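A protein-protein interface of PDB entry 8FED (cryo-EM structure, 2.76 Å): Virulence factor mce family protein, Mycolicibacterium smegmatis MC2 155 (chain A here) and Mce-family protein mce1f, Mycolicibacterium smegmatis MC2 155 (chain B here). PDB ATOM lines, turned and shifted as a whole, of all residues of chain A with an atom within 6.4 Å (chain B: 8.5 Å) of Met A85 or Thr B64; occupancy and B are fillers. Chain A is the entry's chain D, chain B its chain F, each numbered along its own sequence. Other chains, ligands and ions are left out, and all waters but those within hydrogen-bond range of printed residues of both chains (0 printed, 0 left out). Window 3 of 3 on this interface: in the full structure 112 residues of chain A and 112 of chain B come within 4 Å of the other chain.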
ATOM      1  N   ALA A  51       6.650  -0.148 -13.588  1.00  0.00           N
ATOM      2  CA  ALA A  51       7.829  -0.740 -12.980  1.00  0.00           C
ATOM      3  C   ALA A  51       8.175  -2.033 -13.704  1.00  0.00           C
ATOM      4  O   ALA A  51       7.327  -2.659 -14.340  1.00  0.00           O
ATOM      5  CB  ALA A  51       7.619  -1.013 -11.486  1.00  0.00           C
ATOM      6  N   TYR A  52       9.444  -2.420 -13.619  1.00  0.00           N
ATOM      7  CA  TYR A  52       9.934  -3.640 -14.247  1.00  0.00           C
ATOM      8  C   TYR A  52      10.455  -4.585 -13.176  1.00  0.00           C
ATOM      9  O   TYR A  52      11.226  -4.176 -12.303  1.00  0.00           O
ATOM     10  CB  TYR A  52      11.029  -3.336 -15.271  1.00  0.00           C
ATOM     11  CG  TYR A  52      10.510  -2.702 -16.540  1.00  0.00           C
ATOM     12  CD1 TYR A  52      10.029  -3.484 -17.581  1.00  0.00           C
ATOM     13  CD2 TYR A  52      10.500  -1.325 -16.697  1.00  0.00           C
ATOM     14  CE1 TYR A  52       9.552  -2.913 -18.742  1.00  0.00           C
ATOM     15  CE2 TYR A  52      10.026  -0.745 -17.856  1.00  0.00           C
ATOM     16  CZ  TYR A  52       9.553  -1.543 -18.874  1.00  0.00           C
ATOM     17  OH  TYR A  52       9.080  -0.966 -20.030  1.00  0.00           O
ATOM     18  N   PHE A  53      10.037  -5.843 -13.248  1.00  0.00           N
ATOM     19  CA  PHE A  53      10.454  -6.842 -12.279  1.00  0.00           C
ATOM     20  C   PHE A  53      11.070  -8.037 -12.990  1.00  0.00           C
ATOM     21  O   PHE A  53      10.657  -8.386 -14.100  1.00  0.00           O
ATOM     22  CB  PHE A  53       9.270  -7.320 -11.424  1.00  0.00           C
ATOM     23  CG  PHE A  53       8.629  -6.234 -10.605  1.00  0.00           C
ATOM     24  CD1 PHE A  53       7.610  -5.460 -11.132  1.00  0.00           C
ATOM     25  CD2 PHE A  53       9.035  -5.998  -9.305  1.00  0.00           C
ATOM     26  CE1 PHE A  53       7.018  -4.465 -10.380  1.00  0.00           C
ATOM     27  CE2 PHE A  53       8.446  -5.005  -8.551  1.00  0.00           C
ATOM     28  CZ  PHE A  53       7.438  -4.239  -9.089  1.00  0.00           C
ATOM     29  N   PRO A  54      12.080  -8.667 -12.383  1.00  0.00           N
ATOM     30  CA  PRO A  54      12.599  -9.921 -12.951  1.00  0.00           C
ATOM     31  C   PRO A  54      11.566 -11.032 -12.993  1.00  0.00           C
ATOM     32  O   PRO A  54      11.590 -11.857 -13.914  1.00  0.00           O
ATOM     33  CB  PRO A  54      13.771 -10.267 -12.022  1.00  0.00           C
ATOM     34  CG  PRO A  54      13.481  -9.539 -10.752  1.00  0.00           C
ATOM     35  CD  PRO A  54      12.794  -8.274 -11.158  1.00  0.00           C
ATOM     36  N   GLU A  55      10.658 -11.077 -12.021  1.00  0.00           N
ATOM     37  CA  GLU A  55       9.607 -12.081 -11.976  1.00  0.00           C
ATOM     38  C   GLU A  55       8.430 -11.511 -11.200  1.00  0.00           C
ATOM     39  O   GLU A  55       8.620 -10.822 -10.195  1.00  0.00           O
ATOM     40  CB  GLU A  55      10.102 -13.380 -11.330  1.00  0.00           C
ATOM     41  CG  GLU A  55       9.050 -14.469 -11.217  1.00  0.00           C
ATOM     42  CD  GLU A  55       9.571 -15.716 -10.531  1.00  0.00           C
ATOM     43  OE1 GLU A  55      10.774 -15.754 -10.199  1.00  0.00           O
ATOM     44  OE2 GLU A  55       8.777 -16.658 -10.323  1.00  0.00           O
ATOM     45  N   VAL A  56       7.220 -11.798 -11.672  1.00  0.00           N
ATOM     46  CA  VAL A  56       5.987 -11.312 -11.054  1.00  0.00           C
ATOM     47  C   VAL A  56       5.110 -12.539 -10.818  1.00  0.00           C
ATOM     48  O   VAL A  56       4.352 -12.960 -11.697  1.00  0.00           O
ATOM     49  CB  VAL A  56       5.269 -10.267 -11.914  1.00  0.00           C
ATOM     50  CG1 VAL A  56       3.946  -9.880 -11.299  1.00  0.00           C
ATOM     51  CG2 VAL A  56       6.136  -9.039 -12.079  1.00  0.00           C
ATOM     52  N   LEU A  57       5.211 -13.125  -9.629  1.00  0.00           N
ATOM     53  CA  LEU A  57       4.482 -14.335  -9.280  1.00  0.00           C
ATOM     54  C   LEU A  57       3.376 -14.016  -8.283  1.00  0.00           C
ATOM     55  O   LEU A  57       3.585 -13.254  -7.334  1.00  0.00           O
ATOM     56  CB  LEU A  57       5.420 -15.392  -8.691  1.00  0.00           C
ATOM     57  CG  LEU A  57       4.749 -16.655  -8.148  1.00  0.00           C
ATOM     58  CD1 LEU A  57       3.959 -17.349  -9.240  1.00  0.00           C
ATOM     59  CD2 LEU A  57       5.770 -17.600  -7.543  1.00  0.00           C
ATOM     60  N   ALA A  58       2.196 -14.595  -8.523  1.00  0.00           N
ATOM     61  CA  ALA A  58       1.026 -14.463  -7.651  1.00  0.00           C
ATOM     62  C   ALA A  58       0.605 -13.008  -7.476  1.00  0.00           C
ATOM     63  O   ALA A  58      -0.005 -12.643  -6.469  1.00  0.00           O
ATOM     64  CB  ALA A  58       1.262 -15.120  -6.289  1.00  0.00           C
ATOM     65  N   LEU A  59       0.930 -12.169  -8.453  1.00  0.00           N
ATOM     66  CA  LEU A  59       0.487 -10.785  -8.495  1.00  0.00           C
ATOM     67  C   LEU A  59      -0.416 -10.613  -9.706  1.00  0.00           C
ATOM     68  O   LEU A  59      -0.035 -10.978 -10.822  1.00  0.00           O
ATOM     69  CB  LEU A  59       1.675  -9.827  -8.563  1.00  0.00           C
ATOM     70  CG  LEU A  59       1.391  -8.348  -8.326  1.00  0.00           C
ATOM     71  CD1 LEU A  59       0.927  -8.138  -6.901  1.00  0.00           C
ATOM     72  CD2 LEU A  59       2.622  -7.512  -8.620  1.00  0.00           C
ATOM     73  N   ILE A  78      -0.323  -6.212 -15.874  1.00  0.00           N
ATOM     74  CA  ILE A  78       0.963  -6.900 -15.811  1.00  0.00           C
ATOM     75  C   ILE A  78       1.170  -7.628 -17.133  1.00  0.00           C
ATOM     76  O   ILE A  78       0.345  -8.466 -17.513  1.00  0.00           O
ATOM     77  CB  ILE A  78       1.035  -7.898 -14.642  1.00  0.00           C
ATOM     78  CG1 ILE A  78       0.835  -7.183 -13.304  1.00  0.00           C
ATOM     79  CG2 ILE A  78       2.358  -8.647 -14.660  1.00  0.00           C
ATOM     80  CD1 ILE A  78       0.753  -8.109 -12.125  1.00  0.00           C
ATOM     81  N   GLU A  79       2.264  -7.322 -17.830  1.00  0.00           N
ATOM     82  CA  GLU A  79       2.545  -7.944 -19.117  1.00  0.00           C
ATOM     83  C   GLU A  79       4.023  -8.298 -19.210  1.00  0.00           C
ATOM     84  O   GLU A  79       4.846  -7.852 -18.409  1.00  0.00           O
ATOM     85  CB  GLU A  79       2.134  -7.042 -20.290  1.00  0.00           C
ATOM     86  CG  GLU A  79       2.849  -5.701 -20.355  1.00  0.00           C
ATOM     87  CD  GLU A  79       2.175  -4.624 -19.525  1.00  0.00           C
ATOM     88  OE1 GLU A  79       1.334  -4.962 -18.666  1.00  0.00           O
ATOM     89  OE2 GLU A  79       2.479  -3.434 -19.740  1.00  0.00           O
ATOM     90  N   THR A  80       4.348  -9.125 -20.200  1.00  0.00           N
ATOM     91  CA  THR A  80       5.719  -9.558 -20.444  1.00  0.00           C
ATOM     92  C   THR A  80       6.461  -8.491 -21.238  1.00  0.00           C
ATOM     93  O   THR A  80       5.953  -8.006 -22.254  1.00  0.00           O
ATOM     94  CB  THR A  80       5.732 -10.882 -21.204  1.00  0.00           C
ATOM     95  OG1 THR A  80       5.104 -11.898 -20.412  1.00  0.00           O
ATOM     96  CG2 THR A  80       7.156 -11.299 -21.523  1.00  0.00           C
ATOM     97  N   ALA A  81       7.663  -8.120 -20.788  1.00  0.00           N
ATOM     98  CA  ALA A  81       8.478  -7.132 -21.497  1.00  0.00           C
ATOM     99  C   ALA A  81       9.863  -7.740 -21.679  1.00  0.00           C
ATOM    100  O   ALA A  81      10.769  -7.483 -20.883  1.00  0.00           O
ATOM    101  CB  ALA A  81       8.532  -5.811 -20.738  1.00  0.00           C
ATOM    102  N   GLY A  82      10.027  -8.507 -22.757  1.00  0.00           N
ATOM    103  CA  GLY A  82      11.299  -9.168 -22.998  1.00  0.00           C
ATOM    104  C   GLY A  82      11.582 -10.149 -21.881  1.00  0.00           C
ATOM    105  O   GLY A  82      10.733 -10.971 -21.519  1.00  0.00           O
ATOM    106  N   ASP A  83      12.787 -10.079 -21.324  1.00  0.00           N
ATOM    107  CA  ASP A  83      13.111 -10.916 -20.179  1.00  0.00           C
ATOM    108  C   ASP A  83      12.606 -10.331 -18.868  1.00  0.00           C
ATOM    109  O   ASP A  83      12.731 -10.986 -17.828  1.00  0.00           O
ATOM    110  CB  ASP A  83      14.622 -11.138 -20.098  1.00  0.00           C
ATOM    111  CG  ASP A  83      15.395  -9.841 -19.987  1.00  0.00           C
ATOM    112  OD1 ASP A  83      14.901  -8.809 -20.487  1.00  0.00           O
ATOM    113  OD2 ASP A  83      16.498  -9.853 -19.401  1.00  0.00           O
ATOM    114  N   LYS A  84      12.053  -9.123 -18.890  1.00  0.00           N
ATOM    115  CA  LYS A  84      11.496  -8.500 -17.704  1.00  0.00           C
ATOM    116  C   LYS A  84       9.978  -8.683 -17.665  1.00  0.00           C
ATOM    117  O   LYS A  84       9.361  -9.252 -18.578  1.00  0.00           O
ATOM    118  CB  LYS A  84      11.878  -7.019 -17.675  1.00  0.00           C
ATOM    119  CG  LYS A  84      13.363  -6.756 -17.832  1.00  0.00           C
ATOM    120  CD  LYS A  84      13.638  -5.275 -18.022  1.00  0.00           C
ATOM    121  CE  LYS A  84      15.122  -5.005 -18.187  1.00  0.00           C
ATOM    122  NZ  LYS A  84      15.400  -3.556 -18.380  1.00  0.00           N
ATOM    123  N   MET A  85       9.346  -8.062 -16.673  1.00  0.00           N
ATOM    124  CA  MET A  85       7.896  -8.021 -16.575  1.00  0.00           C
ATOM    125  C   MET A  85       7.478  -6.597 -16.252  1.00  0.00           C
ATOM    126  O   MET A  85       7.926  -6.029 -15.251  1.00  0.00           O
ATOM    127  CB  MET A  85       7.401  -8.981 -15.490  1.00  0.00           C
ATOM    128  CG  MET A  85       7.711 -10.445 -15.752  1.00  0.00           C
ATOM    129  SD  MET A  85       6.884 -11.084 -17.212  1.00  0.00           S
ATOM    130  CE  MET A  85       5.203 -10.616 -16.830  1.00  0.00           C
ATOM    131  N   LYS A  86       6.632  -6.031 -17.105  1.00  0.00           N
ATOM    132  CA  LYS A  86       6.195  -4.647 -17.009  1.00  0.00           C
ATOM    133  C   LYS A  86       4.869  -4.606 -16.258  1.00  0.00           C
ATOM    134  O   LYS A  86       3.864  -5.144 -16.735  1.00  0.00           O
ATOM    135  CB  LYS A  86       6.057  -4.040 -18.405  1.00  0.00           C
ATOM    136  CG  LYS A  86       5.425  -2.666 -18.458  1.00  0.00           C
ATOM    137  CD  LYS A  86       5.515  -2.098 -19.868  1.00  0.00           C
ATOM    138  CE  LYS A  86       4.677  -0.843 -20.027  1.00  0.00           C
ATOM    139  NZ  LYS A  86       3.222  -1.146 -19.996  1.00  0.00           N
ATOM    140  N   VAL A  87       4.874  -3.974 -15.088  1.00  0.00           N
ATOM    141  CA  VAL A  87       3.694  -3.849 -14.244  1.00  0.00           C
ATOM    142  C   VAL A  87       3.335  -2.375 -14.163  1.00  0.00           C
ATOM    143  O   VAL A  87       4.136  -1.561 -13.688  1.00  0.00           O
ATOM    144  CB  VAL A  87       3.930  -4.431 -12.842  1.00  0.00           C
ATOM    145  CG1 VAL A  87       2.703  -4.237 -11.973  1.00  0.00           C
ATOM    146  CG2 VAL A  87       4.292  -5.903 -12.933  1.00  0.00           C
ATOM    147  N   ASN B  58      -2.022 -23.908 -13.705  1.00  0.00           N
ATOM    148  CA  ASN B  58      -1.651 -22.754 -14.509  1.00  0.00           C
ATOM    149  C   ASN B  58      -0.277 -22.938 -15.139  1.00  0.00           C
ATOM    150  O   ASN B  58       0.643 -23.483 -14.525  1.00  0.00           O
ATOM    151  CB  ASN B  58      -1.662 -21.487 -13.657  1.00  0.00           C
ATOM    152  CG  ASN B  58      -3.059 -21.039 -13.301  1.00  0.00           C
ATOM    153  OD1 ASN B  58      -3.972 -21.100 -14.124  1.00  0.00           O
ATOM    154  ND2 ASN B  58      -3.238 -20.588 -12.067  1.00  0.00           N
ATOM    155  N   VAL B  59      -0.150 -22.489 -16.383  1.00  0.00           N
ATOM    156  CA  VAL B  59       1.134 -22.345 -17.056  1.00  0.00           C
ATOM    157  C   VAL B  59       1.513 -20.875 -16.998  1.00  0.00           C
ATOM    158  O   VAL B  59       0.700 -20.010 -17.336  1.00  0.00           O
ATOM    159  CB  VAL B  59       1.066 -22.840 -18.511  1.00  0.00           C
ATOM    160  CG1 VAL B  59       2.371 -22.550 -19.231  1.00  0.00           C
ATOM    161  CG2 VAL B  59       0.744 -24.317 -18.553  1.00  0.00           C
ATOM    162  N   THR B  60       2.724 -20.583 -16.539  1.00  0.00           N
ATOM    163  CA  THR B  60       3.147 -19.206 -16.341  1.00  0.00           C
ATOM    164  C   THR B  60       4.445 -18.939 -17.086  1.00  0.00           C
ATOM    165  O   THR B  60       5.233 -19.850 -17.346  1.00  0.00           O
ATOM    166  CB  THR B  60       3.334 -18.877 -14.853  1.00  0.00           C
ATOM    167  OG1 THR B  60       4.280 -19.785 -14.278  1.00  0.00           O
ATOM    168  CG2 THR B  60       2.015 -18.989 -14.107  1.00  0.00           C
ATOM    169  N   TYR B  61       4.638 -17.678 -17.450  1.00  0.00           N
ATOM    170  CA  TYR B  61       5.898 -17.183 -18.000  1.00  0.00           C
ATOM    171  C   TYR B  61       6.397 -16.087 -17.063  1.00  0.00           C
ATOM    172  O   TYR B  61       5.887 -14.962 -17.093  1.00  0.00           O
ATOM    173  CB  TYR B  61       5.725 -16.666 -19.424  1.00  0.00           C
ATOM    174  CG  TYR B  61       7.009 -16.166 -20.047  1.00  0.00           C
ATOM    175  CD1 TYR B  61       7.853 -17.031 -20.729  1.00  0.00           C
ATOM    176  CD2 TYR B  61       7.382 -14.832 -19.947  1.00  0.00           C
ATOM    177  CE1 TYR B  61       9.030 -16.584 -21.293  1.00  0.00           C
ATOM    178  CE2 TYR B  61       8.558 -14.378 -20.507  1.00  0.00           C
ATOM    179  CZ  TYR B  61       9.376 -15.256 -21.179  1.00  0.00           C
ATOM    180  OH  TYR B  61      10.546 -14.800 -21.741  1.00  0.00           O
ATOM    181  N   ARG B  62       7.393 -16.422 -16.239  1.00  0.00           N
ATOM    182  CA  ARG B  62       7.908 -15.529 -15.196  1.00  0.00           C
ATOM    183  C   ARG B  62       6.802 -15.097 -14.236  1.00  0.00           C
ATOM    184  O   ARG B  62       6.756 -13.952 -13.785  1.00  0.00           O
ATOM    185  CB  ARG B  62       8.617 -14.310 -15.793  1.00  0.00           C
ATOM    186  CG  ARG B  62       9.878 -14.644 -16.569  1.00  0.00           C
ATOM    187  CD  ARG B  62      10.671 -13.389 -16.890  1.00  0.00           C
ATOM    188  NE  ARG B  62      11.908 -13.694 -17.597  1.00  0.00           N
ATOM    189  CZ  ARG B  62      13.042 -14.042 -17.007  1.00  0.00           C
ATOM    190  NH1 ARG B  62      13.136 -14.136 -15.691  1.00  0.00           N
ATOM    191  NH2 ARG B  62      14.111 -14.300 -17.755  1.00  0.00           N
ATOM    192  N   GLY B  63       5.901 -16.026 -13.923  1.00  0.00           N
ATOM    193  CA  GLY B  63       4.909 -15.843 -12.891  1.00  0.00           C
ATOM    194  C   GLY B  63       3.529 -15.446 -13.376  1.00  0.00           C
ATOM    195  O   GLY B  63       2.560 -15.626 -12.631  1.00  0.00           O
ATOM    196  N   THR B  64       3.406 -14.924 -14.593  1.00  0.00           N
ATOM    197  CA  THR B  64       2.107 -14.509 -15.107  1.00  0.00           C
ATOM    198  C   THR B  64       1.494 -15.635 -15.929  1.00  0.00           C
ATOM    199  O   THR B  64       2.196 -16.350 -16.649  1.00  0.00           O
ATOM    200  CB  THR B  64       2.213 -13.228 -15.943  1.00  0.00           C
ATOM    201  OG1 THR B  64       0.901 -12.797 -16.322  1.00  0.00           O
ATOM    202  CG2 THR B  64       3.039 -13.447 -17.200  1.00  0.00           C
ATOM    203  N   THR B  65       0.184 -15.812 -15.785  1.00  0.00           N
ATOM    204  CA  THR B  65      -0.495 -16.913 -16.454  1.00  0.00           C
ATOM    205  C   THR B  65      -0.587 -16.669 -17.955  1.00  0.00           C
ATOM    206  O   THR B  65      -0.994 -15.593 -18.401  1.00  0.00           O
ATOM    207  CB  THR B  65      -1.891 -17.107 -15.863  1.00  0.00           C
ATOM    208  OG1 THR B  65      -1.784 -17.345 -14.454  1.00  0.00           O
ATOM    209  CG2 THR B  65      -2.586 -18.292 -16.514  1.00  0.00           C
ATOM    210  N   ILE B  66      -0.200 -17.683 -18.733  1.00  0.00           N
ATOM    211  CA  ILE B  66      -0.246 -17.639 -20.188  1.00  0.00           C
ATOM    212  C   ILE B  66      -0.906 -18.876 -20.773  1.00  0.00           C
ATOM    213  O   ILE B  66      -0.946 -19.022 -21.995  1.00  0.00           O
ATOM    214  CB  ILE B  66       1.159 -17.459 -20.802  1.00  0.00           C
ATOM    215  CG1 ILE B  66       1.997 -18.719 -20.582  1.00  0.00           C
ATOM    216  CG2 ILE B  66       1.863 -16.234 -20.228  1.00  0.00           C
ATOM    217  CD1 ILE B  66       3.313 -18.706 -21.317  1.00  0.00           C
ATOM    218  N   GLY B  67      -1.410 -19.777 -19.940  1.00  0.00           N
ATOM    219  CA  GLY B  67      -2.018 -20.995 -20.434  1.00  0.00           C
ATOM    220  C   GLY B  67      -2.403 -21.894 -19.280  1.00  0.00           C
ATOM    221  O   GLY B  67      -2.361 -21.494 -18.116  1.00  0.00           O
ATOM    222  N   TYR B  86      -1.912 -19.527 -24.898  1.00  0.00           N
ATOM    223  CA  TYR B  86      -2.536 -18.520 -25.746  1.00  0.00           C
ATOM    224  C   TYR B  86      -1.608 -18.131 -26.889  1.00  0.00           C
ATOM    225  O   TYR B  86      -0.403 -17.952 -26.699  1.00  0.00           O
ATOM    226  CB  TYR B  86      -2.901 -17.279 -24.929  1.00  0.00           C
ATOM    227  CG  TYR B  86      -3.962 -17.514 -23.878  1.00  0.00           C
ATOM    228  CD1 TYR B  86      -5.282 -17.742 -24.238  1.00  0.00           C
ATOM    229  CD2 TYR B  86      -3.649 -17.492 -22.528  1.00  0.00           C
ATOM    230  CE1 TYR B  86      -6.257 -17.955 -23.284  1.00  0.00           C
ATOM    231  CE2 TYR B  86      -4.617 -17.704 -21.564  1.00  0.00           C
ATOM    232  CZ  TYR B  86      -5.918 -17.934 -21.949  1.00  0.00           C
ATOM    233  OH  TYR B  86      -6.887 -18.143 -20.996  1.00  0.00           O
ATOM    234  N   ARG B  88      -1.300 -15.403 -28.318  1.00  0.00           N
ATOM    235  CA  ARG B  88      -0.716 -14.081 -28.141  1.00  0.00           C
ATOM    236  C   ARG B  88       0.607 -14.116 -27.387  1.00  0.00           C
ATOM    237  O   ARG B  88       1.315 -13.104 -27.366  1.00  0.00           O
ATOM    238  CB  ARG B  88      -1.694 -13.164 -27.407  1.00  0.00           C
ATOM    239  CG  ARG B  88      -2.182 -13.714 -26.080  1.00  0.00           C
ATOM    240  CD  ARG B  88      -2.994 -12.681 -25.320  1.00  0.00           C
ATOM    241  NE  ARG B  88      -3.583 -13.235 -24.106  1.00  0.00           N
ATOM    242  CZ  ARG B  88      -4.261 -12.529 -23.212  1.00  0.00           C
ATOM    243  NH1 ARG B  88      -4.447 -11.228 -23.357  1.00  0.00           N
ATOM    244  NH2 ARG B  88      -4.764 -13.144 -22.145  1.00  0.00           N
ATOM    245  N   TYR B  89       0.951 -15.244 -26.769  1.00  0.00           N
ATOM    246  CA  TYR B  89       2.199 -15.400 -26.032  1.00  0.00           C
ATOM    247  C   TYR B  89       3.104 -16.374 -26.774  1.00  0.00           C
ATOM    248  O   TYR B  89       2.730 -17.532 -26.993  1.00  0.00           O
ATOM    249  CB  TYR B  89       1.939 -15.894 -24.609  1.00  0.00           C
ATOM    250  CG  TYR B  89       1.347 -14.850 -23.690  1.00  0.00           C
ATOM    251  CD1 TYR B  89       2.119 -13.798 -23.218  1.00  0.00           C
ATOM    252  CD2 TYR B  89       0.021 -14.924 -23.285  1.00  0.00           C
ATOM    253  CE1 TYR B  89       1.586 -12.843 -22.376  1.00  0.00           C
ATOM    254  CE2 TYR B  89      -0.520 -13.974 -22.443  1.00  0.00           C
ATOM    255  CZ  TYR B  89       0.267 -12.936 -21.990  1.00  0.00           C
ATOM    256  OH  TYR B  89      -0.267 -11.986 -21.151  1.00  0.00           O
ATOM    257  N   PHE B 109       2.194 -25.376 -10.108  1.00  0.00           N
ATOM    258  CA  PHE B 109       2.081 -24.839 -11.459  1.00  0.00           C
ATOM    259  C   PHE B 109       3.414 -25.049 -12.165  1.00  0.00           C
ATOM    260  O   PHE B 109       4.352 -25.618 -11.603  1.00  0.00           O
ATOM    261  CB  PHE B 109       1.670 -23.364 -11.440  1.00  0.00           C
ATOM    262  CG  PHE B 109       2.737 -22.437 -10.936  1.00  0.00           C
ATOM    263  CD1 PHE B 109       2.915 -22.237  -9.581  1.00  0.00           C
ATOM    264  CD2 PHE B 109       3.549 -21.747 -11.818  1.00  0.00           C
ATOM    265  CE1 PHE B 109       3.890 -21.380  -9.116  1.00  0.00           C
ATOM    266  CE2 PHE B 109       4.525 -20.891 -11.356  1.00  0.00           C
ATOM    267  CZ  PHE B 109       4.693 -20.707 -10.005  1.00  0.00           C
ATOM    268  N   ILE B 110       3.488 -24.595 -13.414  1.00  0.00           N
ATOM    269  CA  ILE B 110       4.689 -24.728 -14.231  1.00  0.00           C
ATOM    270  C   ILE B 110       5.025 -23.364 -14.820  1.00  0.00           C
ATOM    271  O   ILE B 110       4.138 -22.656 -15.305  1.00  0.00           O
ATOM    272  CB  ILE B 110       4.512 -25.792 -15.333  1.00  0.00           C
ATOM    273  CG1 ILE B 110       5.739 -25.855 -16.241  1.00  0.00           C
ATOM    274  CG2 ILE B 110       3.242 -25.554 -16.131  1.00  0.00           C
ATOM    275  CD1 ILE B 110       5.699 -27.003 -17.217  1.00  0.00           C
ATOM    276  N   ASP B 111       6.300 -22.990 -14.757  1.00  0.00           N
ATOM    277  CA  ASP B 111       6.779 -21.702 -15.232  1.00  0.00           C
ATOM    278  C   ASP B 111       7.724 -21.923 -16.404  1.00  0.00           C
ATOM    279  O   ASP B 111       8.477 -22.899 -16.431  1.00  0.00           O
ATOM    280  CB  ASP B 111       7.488 -20.935 -14.108  1.00  0.00           C
ATOM    281  CG  ASP B 111       7.646 -19.454 -14.409  1.00  0.00           C
ATOM    282  OD1 ASP B 111       7.922 -19.092 -15.571  1.00  0.00           O
ATOM    283  OD2 ASP B 111       7.494 -18.645 -13.471  1.00  0.00           O
ATOM    284  N   LEU B 112       7.673 -21.021 -17.376  1.00  0.00           N
ATOM    285  CA  LEU B 112       8.551 -21.058 -18.541  1.00  0.00           C
ATOM    286  C   LEU B 112       9.564 -19.929 -18.404  1.00  0.00           C
ATOM    287  O   LEU B 112       9.207 -18.753 -18.514  1.00  0.00           O
ATOM    288  CB  LEU B 112       7.744 -20.933 -19.829  1.00  0.00           C
ATOM    289  CG  LEU B 112       6.648 -21.987 -19.990  1.00  0.00           C
ATOM    290  CD1 LEU B 112       5.794 -21.698 -21.209  1.00  0.00           C
ATOM    291  CD2 LEU B 112       7.254 -23.378 -20.071  1.00  0.00           C
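The guanidinium group (NH1) of Arg B62 lies within hydrogen-bond range of the backbone carbonyl oxygen (O) of Pro A54.
The backbone NH (N) of Val A56 lies within hydrogen-bond range of the backbone carbonyl oxygen (O) of Arg B62 (3.1 Å).
The guanidinium group of Arg B62 is in hydrogen-bond range of the backbone carbonyl oxygen of Asp A83 (2.8 Å).
O of Val A56 sits close to O of Gly B63, 3.3 Å away.
The backbone carbonyl oxygen (O) of Phe A53 is in hydrogen-bond range of the backbone NH (N) of Met A85.
OG1 of Thr A80 is in hydrogen-bond range of SD of Met A85 (3.8 Å).
OD1 of Asp B111 is in hydrogen-bond range of N of Arg B62 (2.8 Å).
The side-chain carboxylate (OD2) of Asp B111 is in hydrogen-bond range of the backbone NH (N) of Gly B63, at 3.1 Å.
Of the printed residues of chain B, Pro A54 touches Arg B62.
Of the printed residues of chain B, Glu A55 touches Arg B62 (3.5 Å) and Asp B111 (3.9 Å).
Of the printed residues of chain B, Val A56 touches Arg B62 (3.1 Å), Gly B63 (3.1 Å) and Thr B64 (3.6 Å).
Of the printed residues of chain B, Met A85 touches Arg B62 and Thr B64.
Of the printed residues of chain A, Gly B63 touches Val A56 (3.1 Å) and Leu A57 (3.9 Å).
Of chain A, only Val A56 (3.6 Å) and Met A85 (3.6 Å) come within 4 Å of Thr B64.
The nearest printed residue of chain B that does not touch Met A85 is Tyr B61 (4.01 Å).
The nearest residue of chain A that does not touch Thr B64 is Thr A80 (4.1 Å).
Hydrophobic or aromatic side chains of chain A within 4 Å of the printed part of chain B: Leu A57 and Met A85.
Of the 17 printed residues of chain B, 6 touch a printed residue of chain A.
Hydrophobic or aromatic side chains of chain B within 4 Å of the printed part of chain A: Tyr B61 and Phe B109.
Among the printed residues, 13 pairs touch across the chains.
Among the printed residues, no Asp or Glu carboxylate lies within 4 Å of a Lys or Arg side-chain nitrogen of the other chain.
Among the printed residues, pairs that only touch across the chains: Glu A55 with Arg B62 (3.5 Å), Leu A57 with Phe B109 (3.5 Å), Thr A80 with Tyr B61 (3.5 Å), Met A85 with Thr B64 (3.6 Å), Val A56 with Thr B64 (3.6 Å), Gly A82 with Tyr B61 (3.8 Å), Met A85 with Arg B62 (3.9 Å), Leu A57 with Gly B63 (3.9 Å) and Glu A55 with Asp B111 (3.9 Å).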
